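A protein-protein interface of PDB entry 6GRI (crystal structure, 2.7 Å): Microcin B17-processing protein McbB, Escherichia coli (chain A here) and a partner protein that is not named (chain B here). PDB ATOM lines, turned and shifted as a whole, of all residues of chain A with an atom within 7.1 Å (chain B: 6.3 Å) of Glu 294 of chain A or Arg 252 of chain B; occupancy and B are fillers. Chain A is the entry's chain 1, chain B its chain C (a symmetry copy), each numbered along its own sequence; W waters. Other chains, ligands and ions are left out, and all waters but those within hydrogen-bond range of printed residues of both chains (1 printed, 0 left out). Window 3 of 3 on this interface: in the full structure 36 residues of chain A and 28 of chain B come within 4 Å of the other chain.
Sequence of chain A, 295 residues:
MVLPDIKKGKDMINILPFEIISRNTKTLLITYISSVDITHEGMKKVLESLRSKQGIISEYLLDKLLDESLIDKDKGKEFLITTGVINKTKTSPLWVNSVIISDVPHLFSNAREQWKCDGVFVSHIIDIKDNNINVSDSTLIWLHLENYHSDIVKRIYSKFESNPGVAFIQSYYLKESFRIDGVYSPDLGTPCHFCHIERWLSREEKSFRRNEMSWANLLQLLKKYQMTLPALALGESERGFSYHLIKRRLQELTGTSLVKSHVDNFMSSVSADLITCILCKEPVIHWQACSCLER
Water W1 lies within hydrogen-bond range of the side-chain amide oxygen (OE1) of Gln 288 of chain A (3.0 Å) and the side-chain amino group (NZ) of Lys 24 of chain B (3.0 Å).
CE1 of His 286 of chain A touches OE1 of Gln 251 of chain B, at 3.3 Å. Arg 252 of chain B touches His 286 of chain A. Trp 287 of chain A touches Arg 252 of chain B. OD1 of Asp 250 of chain B touches CD2 of Leu 293 of chain A, at 3.6 Å. Gln 251 of chain B touches Leu 293 of chain A. Arg 252 of chain B touches Leu 293 of chain A.
Hydrophobic or aromatic side chains of chain A within 4 Å of the printed part of chain B: His 286 and Leu 293. Among the printed residues, 9 pairs touch across the chains. Among the printed residues, Asp or Glu carboxylates within 4 Å of a Lys or Arg side-chain nitrogen of the other chain: Glu 294 of chain A with Arg 252 of chain B (3.5 Å).
The backbone carbonyl oxygen of Gln 288 of chain A is in hydrogen-bond range of the guanidinium group of Arg 252 of chain B (3.0 Å). O of Cys 290 of chain A sits at hydrogen-bond distance from NH1 of Arg 252 of chain B, at 3.3 Å. The guanidinium group (NH2) of Arg 252 of chain B is in salt-bridge range of the side-chain carboxylate (OE2) of Glu 294 of chain A.
O of Arg 252 of chain B sits at hydrogen-bond distance from NZ of Lys 24 of chain B, 2.7 Å away. OD2 of Asp 250 of chain B is in salt-bridge range of NH2 of Arg 252 of chain B, 2.6 Å away.
Glu 294 of chain A touches one residue of chain B. Of the printed residues of chain A, Arg 252 of chain B touches His 286, Trp 287, Gln 288, Cys 290, Leu 293 and Glu 294. Printed residues of chain B within 4 Å of Trp 287 of chain A: Arg 252 (3.9 Å). Of the printed residues of chain B, Cys 290 of chain A touches Arg 252. The nearest residue of chain B that does not touch Glu 294 of chain A is Asp 250 of chain B (5.0 Å). The nearest printed residue of chain A that does not touch Asp 250 of chain B is Glu 294 of chain A (5.0 Å).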
ATOM      1  N   HIS A 286      13.812  32.670  13.317  1.00  0.00           N
ATOM      2  CA  HIS A 286      13.410  31.306  12.976  1.00  0.00           C
ATOM      3  C   HIS A 286      13.945  30.317  14.011  1.00  0.00           C
ATOM      4  O   HIS A 286      15.128  30.350  14.355  1.00  0.00           O
ATOM      5  CB  HIS A 286      13.904  30.931  11.578  1.00  0.00           C
ATOM      6  CG  HIS A 286      13.222  31.693  10.489  1.00  0.00           C
ATOM      7  ND1 HIS A 286      13.840  32.706   9.789  1.00  0.00           N
ATOM      8  CD2 HIS A 286      11.956  31.624  10.014  1.00  0.00           C
ATOM      9  CE1 HIS A 286      12.989  33.212   8.912  1.00  0.00           C
ATOM     10  NE2 HIS A 286      11.836  32.579   9.034  1.00  0.00           N
ATOM     11  N   TRP A 287      13.045  29.502  14.558  1.00  0.00           N
ATOM     12  CA  TRP A 287      13.406  28.324  15.372  1.00  0.00           C
ATOM     13  C   TRP A 287      14.152  27.302  14.512  1.00  0.00           C
ATOM     14  O   TRP A 287      13.677  26.910  13.441  1.00  0.00           O
ATOM     15  CB  TRP A 287      12.132  27.704  15.965  1.00  0.00           C
ATOM     16  CG  TRP A 287      12.312  26.554  16.895  1.00  0.00           C
ATOM     17  CD1 TRP A 287      13.309  26.384  17.781  1.00  0.00           C
ATOM     18  CD2 TRP A 287      11.425  25.429  17.060  1.00  0.00           C
ATOM     19  NE1 TRP A 287      13.125  25.209  18.486  1.00  0.00           N
ATOM     20  CE2 TRP A 287      11.969  24.613  18.065  1.00  0.00           C
ATOM     21  CE3 TRP A 287      10.225  25.034  16.450  1.00  0.00           C
ATOM     22  CZ2 TRP A 287      11.368  23.421  18.475  1.00  0.00           C
ATOM     23  CZ3 TRP A 287       9.619  23.839  16.862  1.00  0.00           C
ATOM     24  CH2 TRP A 287      10.197  23.051  17.863  1.00  0.00           C
ATOM     25  N   GLN A 288      15.321  26.886  14.973  1.00  0.00           N
ATOM     26  CA  GLN A 288      16.135  25.917  14.240  1.00  0.00           C
ATOM     27  C   GLN A 288      15.363  24.645  13.828  1.00  0.00           C
ATOM     28  O   GLN A 288      15.532  24.152  12.709  1.00  0.00           O
ATOM     29  CB  GLN A 288      17.407  25.582  15.034  1.00  0.00           C
ATOM     30  CG  GLN A 288      17.173  24.894  16.372  1.00  0.00           C
ATOM     31  CD  GLN A 288      18.253  25.193  17.409  1.00  0.00           C
ATOM     32  OE1 GLN A 288      19.360  25.659  17.086  1.00  0.00           O
ATOM     33  NE2 GLN A 288      17.935  24.916  18.670  1.00  0.00           N
ATOM     34  N   ALA A 289      14.492  24.163  14.712  1.00  0.00           N
ATOM     35  CA  ALA A 289      13.714  22.947  14.474  1.00  0.00           C
ATOM     36  C   ALA A 289      12.461  23.129  13.604  1.00  0.00           C
ATOM     37  O   ALA A 289      11.970  22.162  13.031  1.00  0.00           O
ATOM     38  CB  ALA A 289      13.338  22.287  15.797  1.00  0.00           C
ATOM     39  N   CYS A 290      11.937  24.342  13.501  1.00  0.00           N
ATOM     40  CA  CYS A 290      10.729  24.599  12.694  1.00  0.00           C
ATOM     41  C   CYS A 290      10.957  24.378  11.213  1.00  0.00           C
ATOM     42  O   CYS A 290      12.065  24.537  10.721  1.00  0.00           O
ATOM     43  CB  CYS A 290      10.285  26.033  12.884  1.00  0.00           C
ATOM     44  SG  CYS A 290       8.618  26.381  12.326  1.00  0.00           S
ATOM     45  N   SER A 291       9.897  24.046  10.499  1.00  0.00           N
ATOM     46  CA  SER A 291       9.996  23.731   9.063  1.00  0.00           C
ATOM     47  C   SER A 291       9.429  24.813   8.124  1.00  0.00           C
ATOM     48  O   SER A 291       9.482  24.651   6.903  1.00  0.00           O
ATOM     49  CB  SER A 291       9.305  22.398   8.800  1.00  0.00           C
ATOM     50  OG  SER A 291       8.026  22.379   9.424  1.00  0.00           O
ATOM     51  N   CYS A 292       8.922  25.917   8.669  1.00  0.00           N
ATOM     52  CA  CYS A 292       8.363  26.988   7.843  1.00  0.00           C
ATOM     53  C   CYS A 292       9.260  27.472   6.676  1.00  0.00           C
ATOM     54  O   CYS A 292       8.741  27.887   5.649  1.00  0.00           O
ATOM     55  CB  CYS A 292       7.906  28.185   8.715  1.00  0.00           C
ATOM     56  SG  CYS A 292       9.165  29.027   9.719  1.00  0.00           S
ATOM     57  N   LEU A 293      10.579  27.419   6.829  1.00  0.00           N
ATOM     58  CA  LEU A 293      11.512  27.859   5.777  1.00  0.00           C
ATOM     59  C   LEU A 293      11.619  26.837   4.655  1.00  0.00           C
ATOM     60  O   LEU A 293      11.822  27.201   3.499  1.00  0.00           O
ATOM     61  CB  LEU A 293      12.929  28.076   6.326  1.00  0.00           C
ATOM     62  CG  LEU A 293      13.090  28.998   7.537  1.00  0.00           C
ATOM     63  CD1 LEU A 293      13.327  28.220   8.834  1.00  0.00           C
ATOM     64  CD2 LEU A 293      14.230  29.964   7.295  1.00  0.00           C
ATOM     65  N   GLU A 294      11.524  25.563   5.011  1.00  0.00           N
ATOM     66  CA  GLU A 294      11.700  24.477   4.062  1.00  0.00           C
ATOM     67  C   GLU A 294      10.481  24.292   3.169  1.00  0.00           C
ATOM     68  O   GLU A 294      10.595  23.709   2.089  1.00  0.00           O
ATOM     69  CB  GLU A 294      12.017  23.176   4.794  1.00  0.00           C
ATOM     70  CG  GLU A 294      13.352  23.209   5.529  1.00  0.00           C
ATOM     71  CD  GLU A 294      13.535  22.040   6.475  1.00  0.00           C
ATOM     72  OE1 GLU A 294      12.577  21.698   7.215  1.00  0.00           O
ATOM     73  OE2 GLU A 294      14.653  21.475   6.490  1.00  0.00           O
ATOM     74  N   ARG A 295       9.324  24.771   3.624  1.00  0.00           N
ATOM     75  CA  ARG A 295       8.098  24.730   2.825  1.00  0.00           C
ATOM     76  C   ARG A 295       8.109  25.820   1.755  1.00  0.00           C
ATOM     77  O   ARG A 295       8.790  26.842   1.855  1.00  0.00           O
ATOM     78  CB  ARG A 295       6.844  24.817   3.719  1.00  0.00           C
ATOM     79  CG  ARG A 295       6.643  23.562   4.572  1.00  0.00           C
ATOM     80  CD  ARG A 295       5.184  23.210   4.858  1.00  0.00           C
ATOM     81  NE  ARG A 295       4.821  23.398   6.267  1.00  0.00           N
ATOM     82  CZ  ARG A 295       5.026  22.519   7.258  1.00  0.00           C
ATOM     83  NH1 ARG A 295       5.615  21.333   7.049  1.00  0.00           N
ATOM     84  NH2 ARG A 295       4.636  22.832   8.495  1.00  0.00           N
ATOM     85  OXT ARG A 295       7.445  25.683   0.725  1.00  0.00           O
ATOM     86  N   LEU B  20      25.067  31.505  19.502  1.00  0.00           N
ATOM     87  CA  LEU B  20      24.423  31.587  18.190  1.00  0.00           C
ATOM     88  C   LEU B  20      23.065  32.252  18.314  1.00  0.00           C
ATOM     89  O   LEU B  20      22.745  33.158  17.554  1.00  0.00           O
ATOM     90  CB  LEU B  20      24.269  30.201  17.589  1.00  0.00           C
ATOM     91  CG  LEU B  20      23.706  30.107  16.177  1.00  0.00           C
ATOM     92  CD1 LEU B  20      24.673  30.704  15.155  1.00  0.00           C
ATOM     93  CD2 LEU B  20      23.392  28.656  15.860  1.00  0.00           C
ATOM     94  N   LYS B  24      21.966  35.980  16.665  1.00  0.00           N
ATOM     95  CA  LYS B  24      20.815  36.015  15.759  1.00  0.00           C
ATOM     96  C   LYS B  24      19.698  36.932  16.270  1.00  0.00           C
ATOM     97  O   LYS B  24      19.185  37.735  15.504  1.00  0.00           O
ATOM     98  CB  LYS B  24      20.237  34.617  15.556  1.00  0.00           C
ATOM     99  CG  LYS B  24      21.026  33.680  14.653  1.00  0.00           C
ATOM    100  CD  LYS B  24      20.428  32.288  14.768  1.00  0.00           C
ATOM    101  CE  LYS B  24      20.774  31.417  13.579  1.00  0.00           C
ATOM    102  NZ  LYS B  24      19.956  30.172  13.564  1.00  0.00           N
ATOM    103  N   PHE B 195      26.393  32.439   9.866  1.00  0.00           N
ATOM    104  CA  PHE B 195      26.513  32.752  11.298  1.00  0.00           C
ATOM    105  C   PHE B 195      27.488  31.818  12.013  1.00  0.00           C
ATOM    106  O   PHE B 195      28.423  32.284  12.677  1.00  0.00           O
ATOM    107  CB  PHE B 195      25.151  32.690  12.005  1.00  0.00           C
ATOM    108  CG  PHE B 195      24.187  33.786  11.608  1.00  0.00           C
ATOM    109  CD1 PHE B 195      24.425  35.108  11.963  1.00  0.00           C
ATOM    110  CD2 PHE B 195      23.004  33.488  10.933  1.00  0.00           C
ATOM    111  CE1 PHE B 195      23.521  36.118  11.628  1.00  0.00           C
ATOM    112  CE2 PHE B 195      22.107  34.494  10.586  1.00  0.00           C
ATOM    113  CZ  PHE B 195      22.368  35.810  10.933  1.00  0.00           C
ATOM    114  N   GLU B 196      27.277  30.512  11.852  1.00  0.00           N
ATOM    115  CA  GLU B 196      28.079  29.497  12.555  1.00  0.00           C
ATOM    116  C   GLU B 196      29.575  29.516  12.201  1.00  0.00           C
ATOM    117  O   GLU B 196      30.416  29.243  13.062  1.00  0.00           O
ATOM    118  CB  GLU B 196      27.488  28.098  12.355  1.00  0.00           C
ATOM    119  CG  GLU B 196      26.116  27.929  13.016  1.00  0.00           C
ATOM    120  CD  GLU B 196      25.814  26.503  13.463  1.00  0.00           C
ATOM    121  OE1 GLU B 196      26.709  25.811  13.990  1.00  0.00           O
ATOM    122  OE2 GLU B 196      24.653  26.075  13.298  1.00  0.00           O
ATOM    123  N   LEU B 249      17.910  31.038   0.266  1.00  0.00           N
ATOM    124  CA  LEU B 249      18.784  30.924   1.429  1.00  0.00           C
ATOM    125  C   LEU B 249      17.982  30.471   2.646  1.00  0.00           C
ATOM    126  O   LEU B 249      16.837  30.882   2.838  1.00  0.00           O
ATOM    127  CB  LEU B 249      19.469  32.256   1.698  1.00  0.00           C
ATOM    128  CG  LEU B 249      20.282  32.800   0.522  1.00  0.00           C
ATOM    129  CD1 LEU B 249      20.938  34.111   0.921  1.00  0.00           C
ATOM    130  CD2 LEU B 249      21.317  31.789   0.047  1.00  0.00           C
ATOM    131  N   ASP B 250      18.580  29.588   3.437  1.00  0.00           N
ATOM    132  CA  ASP B 250      18.032  29.184   4.720  1.00  0.00           C
ATOM    133  C   ASP B 250      18.499  30.205   5.757  1.00  0.00           C
ATOM    134  O   ASP B 250      19.688  30.319   6.046  1.00  0.00           O
ATOM    135  CB  ASP B 250      18.536  27.792   5.087  1.00  0.00           C
ATOM    136  CG  ASP B 250      17.667  27.110   6.109  1.00  0.00           C
ATOM    137  OD1 ASP B 250      17.061  27.780   6.980  1.00  0.00           O
ATOM    138  OD2 ASP B 250      17.570  25.872   6.040  1.00  0.00           O
ATOM    139  N   GLN B 251      17.559  30.949   6.319  1.00  0.00           N
ATOM    140  CA  GLN B 251      17.889  32.071   7.218  1.00  0.00           C
ATOM    141  C   GLN B 251      18.426  31.615   8.571  1.00  0.00           C
ATOM    142  O   GLN B 251      19.096  32.389   9.257  1.00  0.00           O
ATOM    143  CB  GLN B 251      16.685  32.993   7.385  1.00  0.00           C
ATOM    144  CG  GLN B 251      16.234  33.598   6.066  1.00  0.00           C
ATOM    145  CD  GLN B 251      14.925  34.321   6.198  1.00  0.00           C
ATOM    146  OE1 GLN B 251      14.807  35.261   6.986  1.00  0.00           O
ATOM    147  NE2 GLN B 251      13.929  33.893   5.430  1.00  0.00           N
ATOM    148  N   ARG B 252      18.155  30.353   8.924  1.00  0.00           N
ATOM    149  CA  ARG B 252      18.722  29.711  10.118  1.00  0.00           C
ATOM    150  C   ARG B 252      20.244  29.568  10.070  1.00  0.00           C
ATOM    151  O   ARG B 252      20.881  29.402  11.108  1.00  0.00           O
ATOM    152  CB  ARG B 252      18.141  28.314  10.292  1.00  0.00           C
ATOM    153  CG  ARG B 252      16.645  28.240  10.522  1.00  0.00           C
ATOM    154  CD  ARG B 252      16.176  26.795  10.488  1.00  0.00           C
ATOM    155  NE  ARG B 252      16.212  26.225   9.137  1.00  0.00           N
ATOM    156  CZ  ARG B 252      15.749  25.016   8.814  1.00  0.00           C
ATOM    157  NH1 ARG B 252      15.193  24.229   9.734  1.00  0.00           N
ATOM    158  NH2 ARG B 252      15.825  24.593   7.559  1.00  0.00           N
ATOM    159  N   THR B 253      20.801  29.592   8.857  1.00  0.00           N
ATOM    160  CA  THR B 253      22.228  29.409   8.602  1.00  0.00           C
ATOM    161  C   THR B 253      22.936  30.664   8.079  1.00  0.00           C
ATOM    162  O   THR B 253      24.083  30.917   8.466  1.00  0.00           O
ATOM    163  CB  THR B 253      22.401  28.237   7.610  1.00  0.00           C
ATOM    164  OG1 THR B 253      22.031  27.024   8.274  1.00  0.00           O
ATOM    165  CG2 THR B 253      23.825  28.100   7.110  1.00  0.00           C
ATOM    166  N   VAL B 254      22.260  31.429   7.221  1.00  0.00           N
ATOM    167  CA  VAL B 254      22.884  32.492   6.441  1.00  0.00           C
ATOM    168  C   VAL B 254      21.929  33.670   6.198  1.00  0.00           C
ATOM    169  O   VAL B 254      20.743  33.487   6.012  1.00  0.00           O
ATOM    170  CB  VAL B 254      23.409  31.933   5.093  1.00  0.00           C
ATOM    171  CG1 VAL B 254      22.300  31.265   4.291  1.00  0.00           C
ATOM    172  CG2 VAL B 254      24.068  33.019   4.259  1.00  0.00           C
HETATM  173  O   HOH W   1      19.710  28.498  16.100  1.00  0.00           O
